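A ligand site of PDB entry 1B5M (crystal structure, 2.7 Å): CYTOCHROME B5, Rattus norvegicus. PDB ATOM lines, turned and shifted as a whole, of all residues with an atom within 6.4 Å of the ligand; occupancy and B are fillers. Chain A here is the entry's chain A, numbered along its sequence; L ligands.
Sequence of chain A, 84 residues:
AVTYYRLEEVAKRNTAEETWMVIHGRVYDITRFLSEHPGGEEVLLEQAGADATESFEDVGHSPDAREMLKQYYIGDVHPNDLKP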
ATOM      1  N   MET A  21      -1.475 -14.420  21.462  1.00  0.00           N
ATOM      2  CA  MET A  21      -0.324 -14.067  20.629  1.00  0.00           C
ATOM      3  C   MET A  21       0.710 -15.172  20.767  1.00  0.00           C
ATOM      4  O   MET A  21       0.790 -15.937  21.721  1.00  0.00           O
ATOM      5  CB  MET A  21       0.376 -12.786  21.166  1.00  0.00           C
ATOM      6  CG  MET A  21       1.202 -11.994  20.145  1.00  0.00           C
ATOM      7  SD  MET A  21       1.060 -10.217  20.541  1.00  0.00           S
ATOM      8  CE  MET A  21       1.274 -10.489  22.319  1.00  0.00           C
ATOM      9  N   ILE A  23       4.725 -15.713  20.690  1.00  0.00           N
ATOM     10  CA  ILE A  23       6.043 -15.082  20.692  1.00  0.00           C
ATOM     11  C   ILE A  23       7.015 -16.216  20.916  1.00  0.00           C
ATOM     12  O   ILE A  23       6.832 -16.898  21.909  1.00  0.00           O
ATOM     13  CB  ILE A  23       6.256 -13.869  21.689  1.00  0.00           C
ATOM     14  CG1 ILE A  23       5.382 -12.645  21.461  1.00  0.00           C
ATOM     15  CG2 ILE A  23       7.673 -13.301  21.657  1.00  0.00           C
ATOM     16  CD1 ILE A  23       5.086 -11.999  22.796  1.00  0.00           C
ATOM     17  N   TYR A  28       0.261 -17.048  24.399  1.00  0.00           N
ATOM     18  CA  TYR A  28      -0.048 -16.261  25.587  1.00  0.00           C
ATOM     19  C   TYR A  28      -1.405 -15.576  25.487  1.00  0.00           C
ATOM     20  O   TYR A  28      -1.917 -15.269  24.401  1.00  0.00           O
ATOM     21  CB  TYR A  28       1.036 -15.204  25.936  1.00  0.00           C
ATOM     22  CG  TYR A  28       2.504 -15.620  25.861  1.00  0.00           C
ATOM     23  CD1 TYR A  28       3.196 -15.579  24.650  1.00  0.00           C
ATOM     24  CD2 TYR A  28       3.209 -16.020  26.999  1.00  0.00           C
ATOM     25  CE1 TYR A  28       4.544 -15.933  24.568  1.00  0.00           C
ATOM     26  CE2 TYR A  28       4.564 -16.373  26.948  1.00  0.00           C
ATOM     27  CZ  TYR A  28       5.234 -16.323  25.718  1.00  0.00           C
ATOM     28  OH  TYR A  28       6.592 -16.634  25.644  1.00  0.00           O
ATOM     29  N   ILE A  30      -2.842 -12.383  26.488  1.00  0.00           N
ATOM     30  CA  ILE A  30      -2.510 -11.020  26.750  1.00  0.00           C
ATOM     31  C   ILE A  30      -3.710 -10.222  27.198  1.00  0.00           C
ATOM     32  O   ILE A  30      -3.632  -9.043  27.540  1.00  0.00           O
ATOM     33  CB  ILE A  30      -2.056 -10.477  25.402  1.00  0.00           C
ATOM     34  CG1 ILE A  30      -0.825 -11.225  24.973  1.00  0.00           C
ATOM     35  CG2 ILE A  30      -1.813  -8.984  25.424  1.00  0.00           C
ATOM     36  CD1 ILE A  30      -1.067 -11.962  23.657  1.00  0.00           C
ATOM     37  N   PHE A  33      -3.116  -7.738  29.854  1.00  0.00           N
ATOM     38  CA  PHE A  33      -1.947  -6.875  29.778  1.00  0.00           C
ATOM     39  C   PHE A  33      -2.112  -5.530  29.076  1.00  0.00           C
ATOM     40  O   PHE A  33      -1.539  -4.557  29.495  1.00  0.00           O
ATOM     41  CB  PHE A  33      -0.905  -7.624  28.985  1.00  0.00           C
ATOM     42  CG  PHE A  33       0.389  -6.880  28.916  1.00  0.00           C
ATOM     43  CD1 PHE A  33       1.057  -6.518  30.095  1.00  0.00           C
ATOM     44  CD2 PHE A  33       0.956  -6.570  27.675  1.00  0.00           C
ATOM     45  CE1 PHE A  33       2.274  -5.853  30.023  1.00  0.00           C
ATOM     46  CE2 PHE A  33       2.171  -5.886  27.576  1.00  0.00           C
ATOM     47  CZ  PHE A  33       2.804  -5.522  28.766  1.00  0.00           C
ATOM     48  N   HIS A  37       0.489  -2.450  28.890  1.00  0.00           N
ATOM     49  CA  HIS A  37       1.403  -2.280  27.762  1.00  0.00           C
ATOM     50  C   HIS A  37       1.718  -0.853  27.445  1.00  0.00           C
ATOM     51  O   HIS A  37       0.903  -0.153  26.843  1.00  0.00           O
ATOM     52  CB  HIS A  37       0.958  -2.811  26.405  1.00  0.00           C
ATOM     53  CG  HIS A  37       2.165  -2.826  25.524  1.00  0.00           C
ATOM     54  ND1 HIS A  37       2.145  -2.456  24.200  1.00  0.00           N
ATOM     55  CD2 HIS A  37       3.423  -3.239  25.819  1.00  0.00           C
ATOM     56  CE1 HIS A  37       3.369  -2.674  23.717  1.00  0.00           C
ATOM     57  NE2 HIS A  37       4.155  -3.163  24.675  1.00  0.00           N
ATOM     58  N   PRO A  38       2.941  -0.511  27.821  1.00  0.00           N
ATOM     59  CA  PRO A  38       3.570   0.811  27.644  1.00  0.00           C
ATOM     60  C   PRO A  38       3.588   1.247  26.148  1.00  0.00           C
ATOM     61  O   PRO A  38       3.320   2.376  25.732  1.00  0.00           O
ATOM     62  CB  PRO A  38       4.981   0.642  28.298  1.00  0.00           C
ATOM     63  CG  PRO A  38       5.012  -0.712  29.021  1.00  0.00           C
ATOM     64  CD  PRO A  38       3.879  -1.535  28.402  1.00  0.00           C
ATOM     65  N   GLY A  39       3.877   0.272  25.291  1.00  0.00           N
ATOM     66  CA  GLY A  39       3.881   0.546  23.877  1.00  0.00           C
ATOM     67  C   GLY A  39       2.475   0.513  23.226  1.00  0.00           C
ATOM     68  O   GLY A  39       2.354   0.435  22.002  1.00  0.00           O
ATOM     69  N   GLY A  40       1.388   0.535  24.015  1.00  0.00           N
ATOM     70  CA  GLY A  40       0.109   0.507  23.323  1.00  0.00           C
ATOM     71  C   GLY A  40      -0.883  -0.659  23.523  1.00  0.00           C
ATOM     72  O   GLY A  40      -0.610  -1.836  23.808  1.00  0.00           O
ATOM     73  N   VAL A  43      -1.497  -1.852  19.339  1.00  0.00           N
ATOM     74  CA  VAL A  43      -0.436  -2.508  18.603  1.00  0.00           C
ATOM     75  C   VAL A  43      -0.614  -4.012  18.629  1.00  0.00           C
ATOM     76  O   VAL A  43      -0.395  -4.690  17.624  1.00  0.00           O
ATOM     77  CB  VAL A  43       0.943  -1.951  19.028  1.00  0.00           C
ATOM     78  CG1 VAL A  43       1.484  -2.497  20.364  1.00  0.00           C
ATOM     79  CG2 VAL A  43       1.967  -1.966  17.904  1.00  0.00           C
ATOM     80  N   LEU A  44      -1.017  -4.490  19.816  1.00  0.00           N
ATOM     81  CA  LEU A  44      -1.287  -5.868  20.161  1.00  0.00           C
ATOM     82  C   LEU A  44      -2.595  -6.338  19.498  1.00  0.00           C
ATOM     83  O   LEU A  44      -2.675  -7.324  18.826  1.00  0.00           O
ATOM     84  CB  LEU A  44      -1.341  -5.992  21.716  1.00  0.00           C
ATOM     85  CG  LEU A  44      -0.141  -5.365  22.521  1.00  0.00           C
ATOM     86  CD1 LEU A  44      -0.310  -5.634  24.019  1.00  0.00           C
ATOM     87  CD2 LEU A  44       1.336  -5.710  22.073  1.00  0.00           C
ATOM     88  N   GLN A  47      -2.432  -7.334  16.390  1.00  0.00           N
ATOM     89  CA  GLN A  47      -1.915  -8.643  15.966  1.00  0.00           C
ATOM     90  C   GLN A  47      -2.430  -9.866  16.750  1.00  0.00           C
ATOM     91  O   GLN A  47      -1.711 -10.873  16.940  1.00  0.00           O
ATOM     92  CB  GLN A  47      -0.368  -8.693  15.827  1.00  0.00           C
ATOM     93  CG  GLN A  47       0.345  -7.412  15.336  1.00  0.00           C
ATOM     94  CD  GLN A  47       1.675  -7.693  14.627  1.00  0.00           C
ATOM     95  OE1 GLN A  47       2.768  -7.414  15.155  1.00  0.00           O
ATOM     96  NE2 GLN A  47       1.591  -8.224  13.409  1.00  0.00           N
ATOM     97  N   ALA A  52       3.399 -12.561  16.941  1.00  0.00           N
ATOM     98  CA  ALA A  52       4.064 -11.324  16.850  1.00  0.00           C
ATOM     99  C   ALA A  52       5.551 -11.430  17.016  1.00  0.00           C
ATOM    100  O   ALA A  52       6.254 -10.463  17.149  1.00  0.00           O
ATOM    101  CB  ALA A  52       3.349 -10.274  17.665  1.00  0.00           C
ATOM    102  N   SER A  55       7.441  -9.052  15.018  1.00  0.00           N
ATOM    103  CA  SER A  55       7.156  -7.714  15.445  1.00  0.00           C
ATOM    104  C   SER A  55       7.758  -7.188  16.757  1.00  0.00           C
ATOM    105  O   SER A  55       8.316  -6.109  16.872  1.00  0.00           O
ATOM    106  CB  SER A  55       6.157  -6.943  14.644  1.00  0.00           C
ATOM    107  OG  SER A  55       5.002  -6.714  15.413  1.00  0.00           O
ATOM    108  N   PHE A  56       7.666  -8.005  17.786  1.00  0.00           N
ATOM    109  CA  PHE A  56       8.172  -7.661  19.096  1.00  0.00           C
ATOM    110  C   PHE A  56       9.684  -7.575  19.095  1.00  0.00           C
ATOM    111  O   PHE A  56      10.291  -6.834  19.847  1.00  0.00           O
ATOM    112  CB  PHE A  56       7.720  -8.799  19.997  1.00  0.00           C
ATOM    113  CG  PHE A  56       8.275  -8.973  21.393  1.00  0.00           C
ATOM    114  CD1 PHE A  56       9.462  -9.676  21.583  1.00  0.00           C
ATOM    115  CD2 PHE A  56       7.517  -8.544  22.489  1.00  0.00           C
ATOM    116  CE1 PHE A  56       9.915  -9.892  22.880  1.00  0.00           C
ATOM    117  CE2 PHE A  56       7.934  -8.758  23.797  1.00  0.00           C
ATOM    118  CZ  PHE A  56       9.147  -9.427  23.973  1.00  0.00           C
ATOM    119  N   VAL A  59      11.009  -4.059  17.601  1.00  0.00           N
ATOM    120  CA  VAL A  59      10.655  -2.925  18.459  1.00  0.00           C
ATOM    121  C   VAL A  59      11.589  -2.884  19.676  1.00  0.00           C
ATOM    122  O   VAL A  59      11.633  -1.976  20.517  1.00  0.00           O
ATOM    123  CB  VAL A  59       9.202  -3.210  18.931  1.00  0.00           C
ATOM    124  CG1 VAL A  59       8.803  -2.449  20.176  1.00  0.00           C
ATOM    125  CG2 VAL A  59       8.170  -2.968  17.848  1.00  0.00           C
ATOM    126  N   GLY A  60      12.357  -3.954  19.762  1.00  0.00           N
ATOM    127  CA  GLY A  60      13.273  -4.103  20.863  1.00  0.00           C
ATOM    128  C   GLY A  60      12.478  -4.109  22.143  1.00  0.00           C
ATOM    129  O   GLY A  60      11.828  -3.125  22.498  1.00  0.00           O
ATOM    130  N   HIS A  61      12.496  -5.253  22.773  1.00  0.00           N
ATOM    131  CA  HIS A  61      11.828  -5.324  24.039  1.00  0.00           C
ATOM    132  C   HIS A  61      12.912  -5.881  24.940  1.00  0.00           C
ATOM    133  O   HIS A  61      13.723  -6.691  24.474  1.00  0.00           O
ATOM    134  CB  HIS A  61      10.511  -6.124  24.088  1.00  0.00           C
ATOM    135  CG  HIS A  61       9.254  -5.495  23.528  1.00  0.00           C
ATOM    136  ND1 HIS A  61       9.066  -5.292  22.164  1.00  0.00           N
ATOM    137  CD2 HIS A  61       8.117  -5.076  24.179  1.00  0.00           C
ATOM    138  CE1 HIS A  61       7.858  -4.752  22.025  1.00  0.00           C
ATOM    139  NE2 HIS A  61       7.254  -4.600  23.210  1.00  0.00           N
ATOM    140  N   SER A  62      12.959  -5.333  26.161  1.00  0.00           N
ATOM    141  CA  SER A  62      13.900  -5.593  27.251  1.00  0.00           C
ATOM    142  C   SER A  62      13.843  -6.990  27.886  1.00  0.00           C
ATOM    143  O   SER A  62      13.068  -7.855  27.519  1.00  0.00           O
ATOM    144  CB  SER A  62      13.623  -4.534  28.318  1.00  0.00           C
ATOM    145  OG  SER A  62      12.640  -5.016  29.226  1.00  0.00           O
ATOM    146  N   PRO A  63      14.693  -7.247  28.876  1.00  0.00           N
ATOM    147  CA  PRO A  63      14.612  -8.540  29.479  1.00  0.00           C
ATOM    148  C   PRO A  63      13.466  -8.495  30.427  1.00  0.00           C
ATOM    149  O   PRO A  63      12.813  -9.504  30.734  1.00  0.00           O
ATOM    150  CB  PRO A  63      15.902  -8.790  30.272  1.00  0.00           C
ATOM    151  CG  PRO A  63      16.769  -7.573  30.083  1.00  0.00           C
ATOM    152  CD  PRO A  63      16.053  -6.694  29.045  1.00  0.00           C
ATOM    153  N   ASP A  64      13.221  -7.290  30.889  1.00  0.00           N
ATOM    154  CA  ASP A  64      12.153  -7.098  31.823  1.00  0.00           C
ATOM    155  C   ASP A  64      10.780  -7.411  31.251  1.00  0.00           C
ATOM    156  O   ASP A  64       9.914  -7.995  31.955  1.00  0.00           O
ATOM    157  CB  ASP A  64      12.287  -5.782  32.617  1.00  0.00           C
ATOM    158  CG  ASP A  64      13.702  -5.608  33.101  1.00  0.00           C
ATOM    159  OD1 ASP A  64      14.671  -6.208  32.632  1.00  0.00           O
ATOM    160  OD2 ASP A  64      13.780  -4.772  34.111  1.00  0.00           O
ATOM    161  N   ALA A  65      10.587  -7.010  29.985  1.00  0.00           N
ATOM    162  CA  ALA A  65       9.329  -7.263  29.270  1.00  0.00           C
ATOM    163  C   ALA A  65       9.209  -8.756  28.962  1.00  0.00           C
ATOM    164  O   ALA A  65       8.119  -9.312  28.789  1.00  0.00           O
ATOM    165  CB  ALA A  65       9.276  -6.532  27.933  1.00  0.00           C
ATOM    166  N   ARG A  66      10.383  -9.371  28.874  1.00  0.00           N
ATOM    167  CA  ARG A  66      10.509 -10.766  28.550  1.00  0.00           C
ATOM    168  C   ARG A  66      10.060 -11.643  29.683  1.00  0.00           C
ATOM    169  O   ARG A  66       9.414 -12.691  29.505  1.00  0.00           O
ATOM    170  CB  ARG A  66      11.941 -11.079  28.139  1.00  0.00           C
ATOM    171  CG  ARG A  66      12.153 -10.825  26.668  1.00  0.00           C
ATOM    172  CD  ARG A  66      13.582 -10.511  26.304  1.00  0.00           C
ATOM    173  NE  ARG A  66      13.661  -9.553  25.210  1.00  0.00           N
ATOM    174  CZ  ARG A  66      13.691  -9.933  23.938  1.00  0.00           C
ATOM    175  NH1 ARG A  66      13.613 -11.199  23.641  1.00  0.00           N
ATOM    176  NH2 ARG A  66      13.776  -9.036  22.945  1.00  0.00           N
ATOM    177  N   MET A  68       8.064 -10.508  31.852  1.00  0.00           N
ATOM    178  CA  MET A  68       6.659 -10.156  31.995  1.00  0.00           C
ATOM    179  C   MET A  68       5.836 -11.091  31.209  1.00  0.00           C
ATOM    180  O   MET A  68       4.677 -11.396  31.511  1.00  0.00           O
ATOM    181  CB  MET A  68       6.394  -8.744  31.459  1.00  0.00           C
ATOM    182  CG  MET A  68       7.154  -7.659  32.223  1.00  0.00           C
ATOM    183  SD  MET A  68       6.113  -6.212  32.496  1.00  0.00           S
ATOM    184  CE  MET A  68       4.485  -7.017  32.414  1.00  0.00           C
ATOM    185  N   LEU A  69       6.505 -11.565  30.186  1.00  0.00           N
ATOM    186  CA  LEU A  69       5.918 -12.510  29.304  1.00  0.00           C
ATOM    187  C   LEU A  69       5.522 -13.786  30.046  1.00  0.00           C
ATOM    188  O   LEU A  69       4.497 -14.422  29.797  1.00  0.00           O
ATOM    189  CB  LEU A  69       6.916 -12.697  28.159  1.00  0.00           C
ATOM    190  CG  LEU A  69       6.253 -12.891  26.817  1.00  0.00           C
ATOM    191  CD1 LEU A  69       5.033 -11.998  26.754  1.00  0.00           C
ATOM    192  CD2 LEU A  69       7.230 -12.411  25.797  1.00  0.00           C
ATOM    193  N   TYR A  72       1.925 -14.430  31.259  1.00  0.00           N
ATOM    194  CA  TYR A  72       0.745 -14.521  30.452  1.00  0.00           C
ATOM    195  C   TYR A  72       0.744 -15.736  29.573  1.00  0.00           C
ATOM    196  O   TYR A  72      -0.016 -15.891  28.627  1.00  0.00           O
ATOM    197  CB  TYR A  72       0.456 -13.218  29.682  1.00  0.00           C
ATOM    198  CG  TYR A  72       0.462 -11.982  30.565  1.00  0.00           C
ATOM    199  CD1 TYR A  72      -0.703 -11.566  31.216  1.00  0.00           C
ATOM    200  CD2 TYR A  72       1.652 -11.275  30.754  1.00  0.00           C
ATOM    201  CE1 TYR A  72      -0.678 -10.456  32.054  1.00  0.00           C
ATOM    202  CE2 TYR A  72       1.713 -10.172  31.601  1.00  0.00           C
ATOM    203  CZ  TYR A  72       0.526  -9.757  32.212  1.00  0.00           C
ATOM    204  OH  TYR A  72       0.563  -8.623  33.003  1.00  0.00           O
HETATM  205  C1  LIG L   1       7.324  -1.247  25.089  1.00  0.00           C
HETATM  206  C2  LIG L   1       6.200  -5.427  27.219  1.00  0.00           C
HETATM  207  C3  LIG L   1       4.367  -6.962  23.005  1.00  0.00           C
HETATM  208  C4  LIG L   1       5.499  -2.781  20.915  1.00  0.00           C
HETATM  209  C5  LIG L   1       7.234  -2.236  26.034  1.00  0.00           C
HETATM  210  C6  LIG L   1       7.792  -2.218  27.374  1.00  0.00           C
HETATM  211  C7  LIG L   1       7.487  -3.381  27.943  1.00  0.00           C
HETATM  212  C8  LIG L   1       6.721  -4.161  26.982  1.00  0.00           C
HETATM  213  C9  LIG L   1       7.815  -3.868  29.354  1.00  0.00           C
HETATM  214  C10 LIG L   1       8.593  -1.029  27.954  1.00  0.00           C
HETATM  215  C11 LIG L   1      10.139  -1.075  27.866  1.00  0.00           C
HETATM  216  C12 LIG L   1      10.769  -2.393  27.551  1.00  0.00           C
HETATM  217  O1  LIG L   1      10.744  -3.236  28.482  1.00  0.00           O
HETATM  218  O2  LIG L   1      11.288  -2.545  26.397  1.00  0.00           O
HETATM  219  C13 LIG L   1       5.573  -6.245  26.259  1.00  0.00           C
HETATM  220  C14 LIG L   1       4.942  -7.555  26.448  1.00  0.00           C
HETATM  221  C15 LIG L   1       4.445  -7.933  25.284  1.00  0.00           C
HETATM  222  C16 LIG L   1       4.737  -6.902  24.334  1.00  0.00           C
HETATM  223  C17 LIG L   1       4.907  -8.321  27.811  1.00  0.00           C
HETATM  224  C18 LIG L   1       3.651  -9.203  24.984  1.00  0.00           C
HETATM  225  C19 LIG L   1       3.074  -9.859  25.987  1.00  0.00           C
HETATM  226  C20 LIG L   1       4.581  -5.998  22.063  1.00  0.00           C
HETATM  227  C21 LIG L   1       4.333  -6.145  20.645  1.00  0.00           C
HETATM  228  C22 LIG L   1       4.655  -4.996  20.083  1.00  0.00           C
HETATM  229  C23 LIG L   1       5.103  -4.092  21.112  1.00  0.00           C
HETATM  230  C24 LIG L   1       3.777  -7.432  19.983  1.00  0.00           C
HETATM  231  C25 LIG L   1       4.561  -4.589  18.604  1.00  0.00           C
HETATM  232  C26 LIG L   1       3.706  -5.260  17.816  1.00  0.00           C
HETATM  233  C27 LIG L   1       5.968  -1.954  21.899  1.00  0.00           C
HETATM  234  C28 LIG L   1       6.154  -0.524  21.809  1.00  0.00           C
HETATM  235  C29 LIG L   1       6.656  -0.127  22.986  1.00  0.00           C
HETATM  236  C30 LIG L   1       6.816  -1.280  23.817  1.00  0.00           C
HETATM  237  C31 LIG L   1       5.825   0.331  20.558  1.00  0.00           C
HETATM  238  C32 LIG L   1       7.026   1.265  23.497  1.00  0.00           C
HETATM  239  C33 LIG L   1       7.532   2.285  22.482  1.00  0.00           C
HETATM  240  C34 LIG L   1       8.885   1.900  22.028  1.00  0.00           C
HETATM  241  O3  LIG L   1       9.695   1.546  22.939  1.00  0.00           O
HETATM  242  O4  LIG L   1       9.068   1.927  20.789  1.00  0.00           O
HETATM  243  N1  LIG L   1       6.588  -3.433  25.807  1.00  0.00           N
HETATM  244  N2  LIG L   1       5.417  -5.865  24.928  1.00  0.00           N
HETATM  245  N3  LIG L   1       5.057  -4.744  22.323  1.00  0.00           N
HETATM  246  N4  LIG L   1       6.387  -2.410  23.152  1.00  0.00           N
HETATM  247 FE1  LIG L   1       5.729  -4.074  24.059  1.00  0.00          FE
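Met 21 touches the ligand (CE to C18, 3.8 Å).
Ile 23 touches the ligand.
CE2 of Phe 33 touches C14 of the ligand, at 3.4 Å.
Pro 38 touches the ligand.
Gly 39 touches the ligand (CA to C29, 3.0 Å).
Val 43 touches the ligand (CG2 to C26, 3.7 Å).
Leu 44 touches the ligand.
OE1 of Gln 47 touches C26 of the ligand, 3.5 Å away.
CB of Ala 52 touches C24 of the ligand, at 3.7 Å.
Ser 55 touches the ligand (OG to C26, 3.1 Å).
Phe 56 touches the ligand.
Val 59 touches the ligand (CG1 to C27, 3.4 Å).
O of Gly 60 touches O2 of the ligand, at 3.98 Å.
CB of Ala 65 touches C2 of the ligand (3.3 Å).
Met 68 touches the ligand.
CD1 of Leu 69 touches C19 of the ligand, at 3.0 Å.
Hydrophobic or aromatic side chains that line the ligand: Met 21, Ile 23, Phe 33, His 37, Pro 38, Val 43, Leu 44, Ala 52, Phe 56, Val 59, His 61, Ala 65, Met 68 and Leu 69.
The nearest printed residue that does not touch the ligand is Ile 30 (4.3 Å).
The side-chain hydroxyl of Ser 62 is in hydrogen-bond range of the backbone NH of Ala 65 (3.0 Å).
The backbone carbonyl oxygen (O) of His 61 is in hydrogen-bond range of the guanidinium group (NH2) of Arg 66 (2.8 Å).
OG of Ser 62 lies within hydrogen-bond range of N of Asp 64 (2.9 Å).
A ring nitrogen (ND1) of His 37 lies close to the backbone NH of Gly 39.
O of Phe 56 lies within hydrogen-bond range of ND1 of His 61 (3.0 Å).
The backbone NH (N) of Tyr 28 lies within hydrogen-bond range of the backbone carbonyl oxygen (O) of Met 21, at 2.9 Å.
O of Gly 40 is in hydrogen-bond range of ND1 of His 37 (2.9 Å).
O of Ser 62 lies within hydrogen-bond range of NE of Arg 66 (2.9 Å).
N of Ser 62 is in hydrogen-bond range of O2 of the ligand (3.3 Å).
A ring nitrogen (NE2) of His 61 is bound to an iron atom (FE1) of the ligand, 1.8 Å away.
NE2 of His 37 is bound to FE1 of the ligand (1.9 Å).
O1 of the ligand sits at hydrogen-bond distance from OG of Ser 62 (2.7 Å).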
